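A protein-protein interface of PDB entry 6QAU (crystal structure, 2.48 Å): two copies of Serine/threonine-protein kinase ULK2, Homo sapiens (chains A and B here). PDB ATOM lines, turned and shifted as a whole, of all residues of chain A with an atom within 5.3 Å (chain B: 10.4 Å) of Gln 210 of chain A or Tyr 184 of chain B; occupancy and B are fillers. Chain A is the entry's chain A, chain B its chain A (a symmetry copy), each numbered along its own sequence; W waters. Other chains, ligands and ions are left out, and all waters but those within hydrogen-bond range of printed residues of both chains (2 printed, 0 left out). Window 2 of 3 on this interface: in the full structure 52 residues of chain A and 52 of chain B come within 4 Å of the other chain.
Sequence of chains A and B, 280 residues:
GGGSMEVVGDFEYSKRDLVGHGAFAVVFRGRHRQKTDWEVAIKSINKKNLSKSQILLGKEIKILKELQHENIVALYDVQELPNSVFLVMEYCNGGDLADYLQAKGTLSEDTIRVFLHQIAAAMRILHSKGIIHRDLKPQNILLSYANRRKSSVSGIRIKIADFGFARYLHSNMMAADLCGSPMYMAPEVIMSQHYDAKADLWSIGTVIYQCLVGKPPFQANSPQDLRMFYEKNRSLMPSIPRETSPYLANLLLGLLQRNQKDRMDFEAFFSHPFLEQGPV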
ATOM      1  N   LEU A 101      -0.187  34.939   5.139  1.00  0.00           N
ATOM      2  CA  LEU A 101      -0.896  35.387   3.935  1.00  0.00           C
ATOM      3  C   LEU A 101      -1.419  36.818   4.098  1.00  0.00           C
ATOM      4  O   LEU A 101      -1.361  37.596   3.158  1.00  0.00           O
ATOM      5  CB  LEU A 101      -2.050  34.434   3.614  1.00  0.00           C
ATOM      6  CG  LEU A 101      -1.650  33.101   2.986  1.00  0.00           C
ATOM      7  CD1 LEU A 101      -2.882  32.356   2.499  1.00  0.00           C
ATOM      8  CD2 LEU A 101      -0.652  33.286   1.840  1.00  0.00           C
ATOM      9  N   GLY A 105       0.055  39.097   1.278  1.00  0.00           N
ATOM     10  CA  GLY A 105      -0.944  39.237   0.232  1.00  0.00           C
ATOM     11  C   GLY A 105      -1.103  37.944  -0.552  1.00  0.00           C
ATOM     12  O   GLY A 105      -2.002  37.169  -0.291  1.00  0.00           O
ATOM     13  N   THR A 106      -0.206  37.734  -1.520  1.00  0.00           N
ATOM     14  CA  THR A 106      -0.172  36.539  -2.319  1.00  0.00           C
ATOM     15  C   THR A 106       1.267  36.081  -2.451  1.00  0.00           C
ATOM     16  O   THR A 106       2.174  36.869  -2.373  1.00  0.00           O
ATOM     17  CB  THR A 106      -0.817  36.736  -3.698  1.00  0.00           C
ATOM     18  OG1 THR A 106      -0.185  37.790  -4.428  1.00  0.00           O
ATOM     19  CG2 THR A 106      -2.291  37.033  -3.588  1.00  0.00           C
ATOM     20  N   LEU A 136      -8.005  20.557   7.370  1.00  0.00           N
ATOM     21  CA  LEU A 136      -6.835  21.366   6.999  1.00  0.00           C
ATOM     22  C   LEU A 136      -7.308  22.741   6.570  1.00  0.00           C
ATOM     23  O   LEU A 136      -8.284  22.876   5.843  1.00  0.00           O
ATOM     24  CB  LEU A 136      -6.068  20.754   5.839  1.00  0.00           C
ATOM     25  CG  LEU A 136      -5.135  19.601   6.164  1.00  0.00           C
ATOM     26  CD1 LEU A 136      -4.551  19.054   4.870  1.00  0.00           C
ATOM     27  CD2 LEU A 136      -4.034  20.045   7.105  1.00  0.00           C
ATOM     28  N   LYS A 137      -6.581  23.755   7.007  1.00  0.00           N
ATOM     29  CA  LYS A 137      -6.898  25.111   6.689  1.00  0.00           C
ATOM     30  C   LYS A 137      -5.704  25.975   7.076  1.00  0.00           C
ATOM     31  O   LYS A 137      -4.775  25.504   7.737  1.00  0.00           O
ATOM     32  CB  LYS A 137      -8.171  25.539   7.425  1.00  0.00           C
ATOM     33  CG  LYS A 137      -8.183  25.253   8.930  1.00  0.00           C
ATOM     34  CD  LYS A 137      -9.544  25.466   9.544  1.00  0.00           C
ATOM     35  CE  LYS A 137      -9.597  25.113  11.006  1.00  0.00           C
ATOM     36  NZ  LYS A 137     -11.008  25.014  11.471  1.00  0.00           N
ATOM     37  N   PRO A 138      -5.659  27.244   6.642  1.00  0.00           N
ATOM     38  CA  PRO A 138      -4.517  28.090   6.939  1.00  0.00           C
ATOM     39  C   PRO A 138      -4.268  28.251   8.446  1.00  0.00           C
ATOM     40  O   PRO A 138      -3.139  28.469   8.837  1.00  0.00           O
ATOM     41  CB  PRO A 138      -4.879  29.417   6.263  1.00  0.00           C
ATOM     42  CG  PRO A 138      -5.880  29.024   5.180  1.00  0.00           C
ATOM     43  CD  PRO A 138      -6.676  27.911   5.819  1.00  0.00           C
ATOM     44  N   GLN A 139      -5.306  28.045   9.263  1.00  0.00           N
ATOM     45  CA  GLN A 139      -5.230  28.233  10.726  1.00  0.00           C
ATOM     46  C   GLN A 139      -4.494  27.062  11.422  1.00  0.00           C
ATOM     47  O   GLN A 139      -4.023  27.241  12.547  1.00  0.00           O
ATOM     48  CB  GLN A 139      -6.623  28.424  11.321  1.00  0.00           C
ATOM     49  CG  GLN A 139      -7.268  29.773  11.001  1.00  0.00           C
ATOM     50  CD  GLN A 139      -7.783  29.869   9.578  1.00  0.00           C
ATOM     51  OE1 GLN A 139      -8.178  28.866   8.956  1.00  0.00           O
ATOM     52  NE2 GLN A 139      -7.803  31.099   9.053  1.00  0.00           N
ATOM     53  N   TRP A 202      -8.707  18.174  -1.454  1.00  0.00           N
ATOM     54  CA  TRP A 202      -9.552  19.323  -1.731  1.00  0.00           C
ATOM     55  C   TRP A 202      -9.060  20.511  -0.908  1.00  0.00           C
ATOM     56  O   TRP A 202      -8.910  21.614  -1.424  1.00  0.00           O
ATOM     57  CB  TRP A 202     -11.021  19.037  -1.432  1.00  0.00           C
ATOM     58  CG  TRP A 202     -11.878  20.266  -1.457  1.00  0.00           C
ATOM     59  CD1 TRP A 202     -12.092  21.130  -0.425  1.00  0.00           C
ATOM     60  CD2 TRP A 202     -12.630  20.781  -2.565  1.00  0.00           C
ATOM     61  NE1 TRP A 202     -12.934  22.135  -0.808  1.00  0.00           N
ATOM     62  CE2 TRP A 202     -13.266  21.955  -2.119  1.00  0.00           C
ATOM     63  CE3 TRP A 202     -12.837  20.369  -3.885  1.00  0.00           C
ATOM     64  CZ2 TRP A 202     -14.068  22.731  -2.952  1.00  0.00           C
ATOM     65  CZ3 TRP A 202     -13.642  21.130  -4.697  1.00  0.00           C
ATOM     66  CH2 TRP A 202     -14.251  22.293  -4.240  1.00  0.00           C
ATOM     67  N   SER A 203      -8.828  20.274   0.378  1.00  0.00           N
ATOM     68  CA  SER A 203      -8.457  21.312   1.319  1.00  0.00           C
ATOM     69  C   SER A 203      -7.187  22.022   0.838  1.00  0.00           C
ATOM     70  O   SER A 203      -7.123  23.247   0.807  1.00  0.00           O
ATOM     71  CB  SER A 203      -8.256  20.727   2.736  1.00  0.00           C
ATOM     72  OG  SER A 203      -9.486  20.330   3.294  1.00  0.00           O
ATOM     73  N   GLY A 205      -6.047  22.100  -2.043  1.00  0.00           N
ATOM     74  CA  GLY A 205      -6.450  22.843  -3.211  1.00  0.00           C
ATOM     75  C   GLY A 205      -6.928  24.234  -2.858  1.00  0.00           C
ATOM     76  O   GLY A 205      -6.526  25.208  -3.504  1.00  0.00           O
ATOM     77  N   THR A 206      -7.818  24.330  -1.864  1.00  0.00           N
ATOM     78  CA  THR A 206      -8.383  25.617  -1.456  1.00  0.00           C
ATOM     79  C   THR A 206      -7.283  26.526  -0.902  1.00  0.00           C
ATOM     80  O   THR A 206      -7.330  27.725  -1.087  1.00  0.00           O
ATOM     81  CB  THR A 206      -9.515  25.457  -0.440  1.00  0.00           C
ATOM     82  OG1 THR A 206      -9.009  24.802   0.731  1.00  0.00           O
ATOM     83  CG2 THR A 206     -10.679  24.688  -1.020  1.00  0.00           C
ATOM     84  N   VAL A 207      -6.289  25.925  -0.243  1.00  0.00           N
ATOM     85  CA  VAL A 207      -5.258  26.664   0.452  1.00  0.00           C
ATOM     86  C   VAL A 207      -4.256  27.203  -0.571  1.00  0.00           C
ATOM     87  O   VAL A 207      -3.833  28.346  -0.485  1.00  0.00           O
ATOM     88  CB  VAL A 207      -4.567  25.797   1.525  1.00  0.00           C
ATOM     89  CG1 VAL A 207      -3.256  26.418   2.024  1.00  0.00           C
ATOM     90  CG2 VAL A 207      -5.485  25.527   2.690  1.00  0.00           C
ATOM     91  N   ILE A 208      -3.836  26.346  -1.496  1.00  0.00           N
ATOM     92  CA  ILE A 208      -2.941  26.766  -2.570  1.00  0.00           C
ATOM     93  C   ILE A 208      -3.609  27.884  -3.373  1.00  0.00           C
ATOM     94  O   ILE A 208      -2.983  28.853  -3.720  1.00  0.00           O
ATOM     95  CB  ILE A 208      -2.573  25.597  -3.489  1.00  0.00           C
ATOM     96  CG1 ILE A 208      -1.764  24.521  -2.773  1.00  0.00           C
ATOM     97  CG2 ILE A 208      -1.833  26.110  -4.686  1.00  0.00           C
ATOM     98  CD1 ILE A 208      -0.917  25.035  -1.641  1.00  0.00           C
ATOM     99  N   TYR A 209      -4.888  27.703  -3.689  1.00  0.00           N
ATOM    100  CA  TYR A 209      -5.609  28.668  -4.452  1.00  0.00           C
ATOM    101  C   TYR A 209      -5.545  30.014  -3.737  1.00  0.00           C
ATOM    102  O   TYR A 209      -5.340  31.015  -4.365  1.00  0.00           O
ATOM    103  CB  TYR A 209      -7.044  28.213  -4.674  1.00  0.00           C
ATOM    104  CG  TYR A 209      -7.875  29.166  -5.482  1.00  0.00           C
ATOM    105  CD1 TYR A 209      -8.438  30.289  -4.901  1.00  0.00           C
ATOM    106  CD2 TYR A 209      -8.095  28.959  -6.830  1.00  0.00           C
ATOM    107  CE1 TYR A 209      -9.204  31.182  -5.629  1.00  0.00           C
ATOM    108  CE2 TYR A 209      -8.866  29.839  -7.577  1.00  0.00           C
ATOM    109  CZ  TYR A 209      -9.422  30.957  -6.976  1.00  0.00           C
ATOM    110  OH  TYR A 209     -10.193  31.830  -7.690  1.00  0.00           O
ATOM    111  N   GLN A 210      -5.708  30.014  -2.418  1.00  0.00           N
ATOM    112  CA  GLN A 210      -5.731  31.249  -1.646  1.00  0.00           C
ATOM    113  C   GLN A 210      -4.339  31.887  -1.606  1.00  0.00           C
ATOM    114  O   GLN A 210      -4.214  33.097  -1.619  1.00  0.00           O
ATOM    115  CB  GLN A 210      -6.264  31.016  -0.233  1.00  0.00           C
ATOM    116  CG  GLN A 210      -6.111  32.255   0.624  1.00  0.00           C
ATOM    117  CD  GLN A 210      -6.902  32.222   1.903  1.00  0.00           C
ATOM    118  OE1 GLN A 210      -7.903  31.521   2.039  1.00  0.00           O
ATOM    119  NE2 GLN A 210      -6.462  33.027   2.848  1.00  0.00           N
ATOM    120  N   CYS A 211      -3.296  31.071  -1.548  1.00  0.00           N
ATOM    121  CA  CYS A 211      -1.914  31.574  -1.637  1.00  0.00           C
ATOM    122  C   CYS A 211      -1.698  32.320  -2.973  1.00  0.00           C
ATOM    123  O   CYS A 211      -1.080  33.379  -3.010  1.00  0.00           O
ATOM    124  CB  CYS A 211      -0.907  30.437  -1.513  1.00  0.00           C
ATOM    125  SG  CYS A 211      -0.883  29.701   0.141  1.00  0.00           S
ATOM    126  N   LEU A 212      -2.209  31.739  -4.068  1.00  0.00           N
ATOM    127  CA  LEU A 212      -1.988  32.238  -5.422  1.00  0.00           C
ATOM    128  C   LEU A 212      -2.828  33.494  -5.666  1.00  0.00           C
ATOM    129  O   LEU A 212      -2.321  34.462  -6.196  1.00  0.00           O
ATOM    130  CB  LEU A 212      -2.352  31.136  -6.419  1.00  0.00           C
ATOM    131  CG  LEU A 212      -2.077  31.431  -7.889  1.00  0.00           C
ATOM    132  CD1 LEU A 212      -0.585  31.540  -8.150  1.00  0.00           C
ATOM    133  CD2 LEU A 212      -2.705  30.357  -8.766  1.00  0.00           C
ATOM    134  N   VAL A 213      -4.094  33.461  -5.259  1.00  0.00           N
ATOM    135  CA  VAL A 213      -5.091  34.386  -5.755  1.00  0.00           C
ATOM    136  C   VAL A 213      -5.385  35.452  -4.690  1.00  0.00           C
ATOM    137  O   VAL A 213      -5.798  36.527  -5.022  1.00  0.00           O
ATOM    138  CB  VAL A 213      -6.373  33.623  -6.156  1.00  0.00           C
ATOM    139  CG1 VAL A 213      -7.524  34.542  -6.521  1.00  0.00           C
ATOM    140  CG2 VAL A 213      -6.103  32.640  -7.267  1.00  0.00           C
ATOM    141  N   GLY A 214      -5.225  35.109  -3.408  1.00  0.00           N
ATOM    142  CA  GLY A 214      -5.467  36.041  -2.305  1.00  0.00           C
ATOM    143  C   GLY A 214      -6.846  35.886  -1.683  1.00  0.00           C
ATOM    144  O   GLY A 214      -7.169  36.591  -0.767  1.00  0.00           O
ATOM    145  N   LYS A 215      -7.665  34.958  -2.184  1.00  0.00           N
ATOM    146  CA  LYS A 215      -8.919  34.604  -1.516  1.00  0.00           C
ATOM    147  C   LYS A 215      -9.207  33.130  -1.746  1.00  0.00           C
ATOM    148  O   LYS A 215      -8.624  32.524  -2.624  1.00  0.00           O
ATOM    149  CB  LYS A 215     -10.075  35.458  -2.025  1.00  0.00           C
ATOM    150  CG  LYS A 215     -10.182  36.826  -1.372  1.00  0.00           C
ATOM    151  CD  LYS A 215     -11.473  37.582  -1.696  1.00  0.00           C
ATOM    152  CE  LYS A 215     -11.322  39.090  -1.582  1.00  0.00           C
ATOM    153  NZ  LYS A 215     -12.364  39.810  -2.353  1.00  0.00           N
ATOM    154  N   PRO A 216     -10.052  32.484  -0.923  1.00  0.00           N
ATOM    155  CA  PRO A 216     -10.441  31.099  -1.160  1.00  0.00           C
ATOM    156  C   PRO A 216     -11.310  31.004  -2.409  1.00  0.00           C
ATOM    157  O   PRO A 216     -11.889  31.995  -2.830  1.00  0.00           O
ATOM    158  CB  PRO A 216     -11.251  30.687   0.073  1.00  0.00           C
ATOM    159  CG  PRO A 216     -11.130  31.852   1.045  1.00  0.00           C
ATOM    160  CD  PRO A 216     -10.707  33.063   0.247  1.00  0.00           C
ATOM    161  N   PRO A 217     -11.385  29.832  -3.073  1.00  0.00           N
ATOM    162  CA  PRO A 217     -12.047  29.725  -4.369  1.00  0.00           C
ATOM    163  C   PRO A 217     -13.577  29.794  -4.295  1.00  0.00           C
ATOM    164  O   PRO A 217     -14.205  30.194  -5.260  1.00  0.00           O
ATOM    165  CB  PRO A 217     -11.582  28.367  -4.906  1.00  0.00           C
ATOM    166  CG  PRO A 217     -11.245  27.573  -3.673  1.00  0.00           C
ATOM    167  CD  PRO A 217     -10.746  28.583  -2.669  1.00  0.00           C
ATOM    168  N   ALA B 175     -19.853  19.041  11.868  1.00  0.00           N
ATOM    169  CA  ALA B 175     -18.633  19.475  11.154  1.00  0.00           C
ATOM    170  C   ALA B 175     -18.378  20.979  11.378  1.00  0.00           C
ATOM    171  O   ALA B 175     -17.251  21.380  11.657  1.00  0.00           O
ATOM    172  CB  ALA B 175     -18.753  19.144   9.680  1.00  0.00           C
ATOM    173  N   CYS B 179     -15.464  22.583  14.127  1.00  0.00           N
ATOM    174  CA  CYS B 179     -14.309  22.792  13.229  1.00  0.00           C
ATOM    175  C   CYS B 179     -14.337  24.184  12.573  1.00  0.00           C
ATOM    176  O   CYS B 179     -13.652  24.413  11.547  1.00  0.00           O
ATOM    177  CB  CYS B 179     -14.254  21.712  12.155  1.00  0.00           C
ATOM    178  SG  CYS B 179     -13.555  20.152  12.750  1.00  0.00           S
ATOM    179  N   GLY B 180     -15.101  25.110  13.166  1.00  0.00           N
ATOM    180  CA  GLY B 180     -15.101  26.516  12.758  1.00  0.00           C
ATOM    181  C   GLY B 180     -15.588  26.692  11.326  1.00  0.00           C
ATOM    182  O   GLY B 180     -16.444  25.912  10.845  1.00  0.00           O
ATOM    183  N   SER B 181     -15.045  27.715  10.647  1.00  0.00           N
ATOM    184  CA  SER B 181     -15.407  28.013   9.259  1.00  0.00           C
ATOM    185  C   SER B 181     -15.073  26.817   8.378  1.00  0.00           C
ATOM    186  O   SER B 181     -13.950  26.314   8.433  1.00  0.00           O
ATOM    187  CB  SER B 181     -14.731  29.242   8.734  1.00  0.00           C
ATOM    188  OG  SER B 181     -15.182  29.518   7.416  1.00  0.00           O
ATOM    189  N   PRO B 182     -16.017  26.370   7.512  1.00  0.00           N
ATOM    190  CA  PRO B 182     -15.832  25.174   6.698  1.00  0.00           C
ATOM    191  C   PRO B 182     -15.294  25.470   5.289  1.00  0.00           C
ATOM    192  O   PRO B 182     -15.439  24.644   4.397  1.00  0.00           O
ATOM    193  CB  PRO B 182     -17.278  24.663   6.632  1.00  0.00           C
ATOM    194  CG  PRO B 182     -18.095  25.946   6.491  1.00  0.00           C
ATOM    195  CD  PRO B 182     -17.319  27.007   7.250  1.00  0.00           C
ATOM    196  N   MET B 183     -14.653  26.627   5.110  1.00  0.00           N
ATOM    197  CA  MET B 183     -14.371  27.152   3.797  1.00  0.00           C
ATOM    198  C   MET B 183     -13.301  26.317   3.080  1.00  0.00           C
ATOM    199  O   MET B 183     -13.211  26.348   1.867  1.00  0.00           O
ATOM    200  CB  MET B 183     -13.894  28.601   3.885  1.00  0.00           C
ATOM    201  CG  MET B 183     -15.029  29.605   3.916  1.00  0.00           C
ATOM    202  SD  MET B 183     -14.461  31.136   3.217  1.00  0.00           S
ATOM    203  CE  MET B 183     -12.929  31.377   4.129  1.00  0.00           C
ATOM    204  N   TYR B 184     -12.498  25.583   3.860  1.00  0.00           N
ATOM    205  CA  TYR B 184     -11.385  24.816   3.354  1.00  0.00           C
ATOM    206  C   TYR B 184     -11.698  23.314   3.420  1.00  0.00           C
ATOM    207  O   TYR B 184     -10.883  22.461   3.128  1.00  0.00           O
ATOM    208  CB  TYR B 184     -10.143  25.187   4.151  1.00  0.00           C
ATOM    209  CG  TYR B 184      -9.869  26.660   4.172  1.00  0.00           C
ATOM    210  CD1 TYR B 184     -10.353  27.457   5.186  1.00  0.00           C
ATOM    211  CD2 TYR B 184      -9.165  27.272   3.144  1.00  0.00           C
ATOM    212  CE1 TYR B 184     -10.099  28.822   5.212  1.00  0.00           C
ATOM    213  CE2 TYR B 184      -8.899  28.634   3.157  1.00  0.00           C
ATOM    214  CZ  TYR B 184      -9.371  29.416   4.193  1.00  0.00           C
ATOM    215  OH  TYR B 184      -9.100  30.747   4.201  1.00  0.00           O
ATOM    216  N   MET B 185     -12.894  22.997   3.864  1.00  0.00           N
ATOM    217  CA  MET B 185     -13.285  21.650   4.182  1.00  0.00           C
ATOM    218  C   MET B 185     -13.823  20.999   2.896  1.00  0.00           C
ATOM    219  O   MET B 185     -14.483  21.635   2.102  1.00  0.00           O
ATOM    220  CB  MET B 185     -14.356  21.714   5.281  1.00  0.00           C
ATOM    221  CG  MET B 185     -14.685  20.433   5.910  1.00  0.00           C
ATOM    222  SD  MET B 185     -15.717  20.682   7.424  1.00  0.00           S
ATOM    223  CE  MET B 185     -14.499  21.194   8.637  1.00  0.00           C
ATOM    224  N   ALA B 186     -13.513  19.718   2.704  1.00  0.00           N
ATOM    225  CA  ALA B 186     -13.954  18.981   1.537  1.00  0.00           C
ATOM    226  C   ALA B 186     -15.470  18.938   1.492  1.00  0.00           C
ATOM    227  O   ALA B 186     -16.116  18.768   2.513  1.00  0.00           O
ATOM    228  CB  ALA B 186     -13.399  17.587   1.564  1.00  0.00           C
ATOM    229  N   PRO B 187     -16.091  19.046   0.294  1.00  0.00           N
ATOM    230  CA  PRO B 187     -17.548  18.980   0.176  1.00  0.00           C
ATOM    231  C   PRO B 187     -18.152  17.703   0.761  1.00  0.00           C
ATOM    232  O   PRO B 187     -19.206  17.761   1.373  1.00  0.00           O
ATOM    233  CB  PRO B 187     -17.780  19.067  -1.335  1.00  0.00           C
ATOM    234  CG  PRO B 187     -16.593  19.876  -1.800  1.00  0.00           C
ATOM    235  CD  PRO B 187     -15.440  19.329  -0.991  1.00  0.00           C
ATOM    236  N   GLU B 188     -17.470  16.577   0.581  1.00  0.00           N
ATOM    237  CA  GLU B 188     -18.006  15.321   1.063  1.00  0.00           C
ATOM    238  C   GLU B 188     -17.962  15.294   2.616  1.00  0.00           C
ATOM    239  O   GLU B 188     -18.758  14.646   3.234  1.00  0.00           O
ATOM    240  CB  GLU B 188     -17.281  14.139   0.417  1.00  0.00           C
ATOM    241  CG  GLU B 188     -15.813  14.015   0.785  1.00  0.00           C
ATOM    242  CD  GLU B 188     -14.832  14.693  -0.152  1.00  0.00           C
ATOM    243  OE1 GLU B 188     -15.280  15.582  -0.898  1.00  0.00           O
ATOM    244  OE2 GLU B 188     -13.617  14.265  -0.155  1.00  0.00           O
ATOM    245  N   VAL B 189     -17.047  16.031   3.239  1.00  0.00           N
ATOM    246  CA  VAL B 189     -17.016  16.139   4.681  1.00  0.00           C
ATOM    247  C   VAL B 189     -18.125  17.101   5.175  1.00  0.00           C
ATOM    248  O   VAL B 189     -18.807  16.806   6.136  1.00  0.00           O
ATOM    249  CB  VAL B 189     -15.624  16.562   5.174  1.00  0.00           C
ATOM    250  CG1 VAL B 189     -15.613  16.862   6.667  1.00  0.00           C
ATOM    251  CG2 VAL B 189     -14.584  15.512   4.853  1.00  0.00           C
ATOM    252  N   ILE B 190     -18.302  18.245   4.512  1.00  0.00           N
ATOM    253  CA  ILE B 190     -19.330  19.214   4.863  1.00  0.00           C
ATOM    254  C   ILE B 190     -20.718  18.563   4.751  1.00  0.00           C
ATOM    255  O   ILE B 190     -21.610  18.866   5.510  1.00  0.00           O
ATOM    256  CB  ILE B 190     -19.229  20.458   3.971  1.00  0.00           C
ATOM    257  CG1 ILE B 190     -17.972  21.262   4.278  1.00  0.00           C
ATOM    258  CG2 ILE B 190     -20.467  21.331   4.080  1.00  0.00           C
ATOM    259  CD1 ILE B 190     -17.770  22.431   3.347  1.00  0.00           C
HETATM  260  O   HOH W   1     -14.573  24.171   0.877  1.00  0.00           O
HETATM  261  O   HOH W   2     -11.899  18.196   4.640  1.00  0.00           O
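O of Leu 136 of chain A touches CB of Tyr 184 of chain B, 3.4 Å away. CB of Lys 137 of chain A touches CD1 of Tyr 184 of chain B, 3.7 Å away. Tyr 184 of chain B touches Pro 138 of chain A (CZ to CD, 3.5 Å). Trp 202 of chain A touches Tyr 184 of chain B (CD1 to O, 3.98 Å). CD1 of Trp 202 of chain A touches CA of Ala 186 of chain B (3.5 Å). Trp 202 of chain A touches Pro 187 of chain B (CD2 to CD, 3.5 Å). CD2 of Tyr 184 of chain B touches OG1 of Thr 206 of chain A, 3.5 Å away. CG of Pro 216 of chain A touches CE of Met 183 of chain B, at 3.6 Å. OH of Tyr 184 of chain B touches CG of Pro 216 of chain A, at 3.9 Å.
Of the 13 printed residues of chain B, 6 touch a printed residue of chain A. Hydrophobic or aromatic side chains of chain B that line the printed part of chain A: Met 183, Tyr 184 and Pro 187. Hydrophobic or aromatic side chains of chain A that line the printed part of chain B: Pro 138, Trp 202 and Pro 216. Among the printed residues, 13 pairs touch across the chains.
Water W1 lies within hydrogen-bond range of O of Met 183 of chain B, O of Met 185 of chain B and NE1 of Trp 202 of chain A. Water W2 lies within hydrogen-bond range of the backbone NH (N) of Ala 186 of chain B (2.9 Å) and the side-chain hydroxyl (OG) of Ser 203 of chain A (3.5 Å).
No position is printed for both chains.
Of the printed residues of chain B, Leu 136 of chain A touches Tyr 184 (3.4 Å). Printed residues of chain B within 4 Å of Trp 202 of chain A: Tyr 184, Met 185, Ala 186 and Pro 187. Of chain B, only Tyr 184 comes within 4 Å of Ser 203 of chain A. Thr 206 of chain A touches just one residue of chain B: Tyr 184 (3.5 Å). No residue of chain B comes within 4 Å of Val 207 of chain A. Gln 210 of chain A touches one residue of chain B. Cys 211 of chain A touches none of the printed residues of chain B. No residue of chain B comes within 4 Å of Val 213 of chain A. No residue of chain B comes within 4 Å of Gly 214 of chain A. Lys 215 of chain A touches none of the printed residues of chain B. Pro 216 of chain A touches just these residues of chain B: Met 183 and Tyr 184. Of the printed residues of chain A, Met 183 of chain B touches Pro 216. Printed residues of chain A within 4 Å of Tyr 184 of chain B: Leu 136, Lys 137, Pro 138, Trp 202, Ser 203, Thr 206, Gln 210 and Pro 216. Of the printed residues of chain A, Ala 186 of chain B touches Trp 202. Glu 188 of chain B touches none of the printed residues of chain A. The nearest printed residue of chain A that does not touch Tyr 184 of chain B is Val 207 of chain A (4.1 Å).
The backbone carbonyl oxygen (O) of Tyr 184 of chain B sits at hydrogen-bond distance from the side-chain hydroxyl (OG) of Ser 203 of chain A. OE1 of Gln 210 of chain A sits at hydrogen-bond distance from OH of Tyr 184 of chain B. The side-chain amino group (NZ) of Lys 137 of chain A sits at hydrogen-bond distance from the backbone carbonyl oxygen (O) of Cys 179 of chain B (2.7 Å). The backbone carbonyl oxygen (O) of Met 185 of chain B is in hydrogen-bond range of the indole nitrogen (NE1) of Trp 202 of chain A (3.3 Å).
O of Ser 203 of chain A sits at hydrogen-bond distance from OG1 of Thr 206 of chain A, at 2.4 Å.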
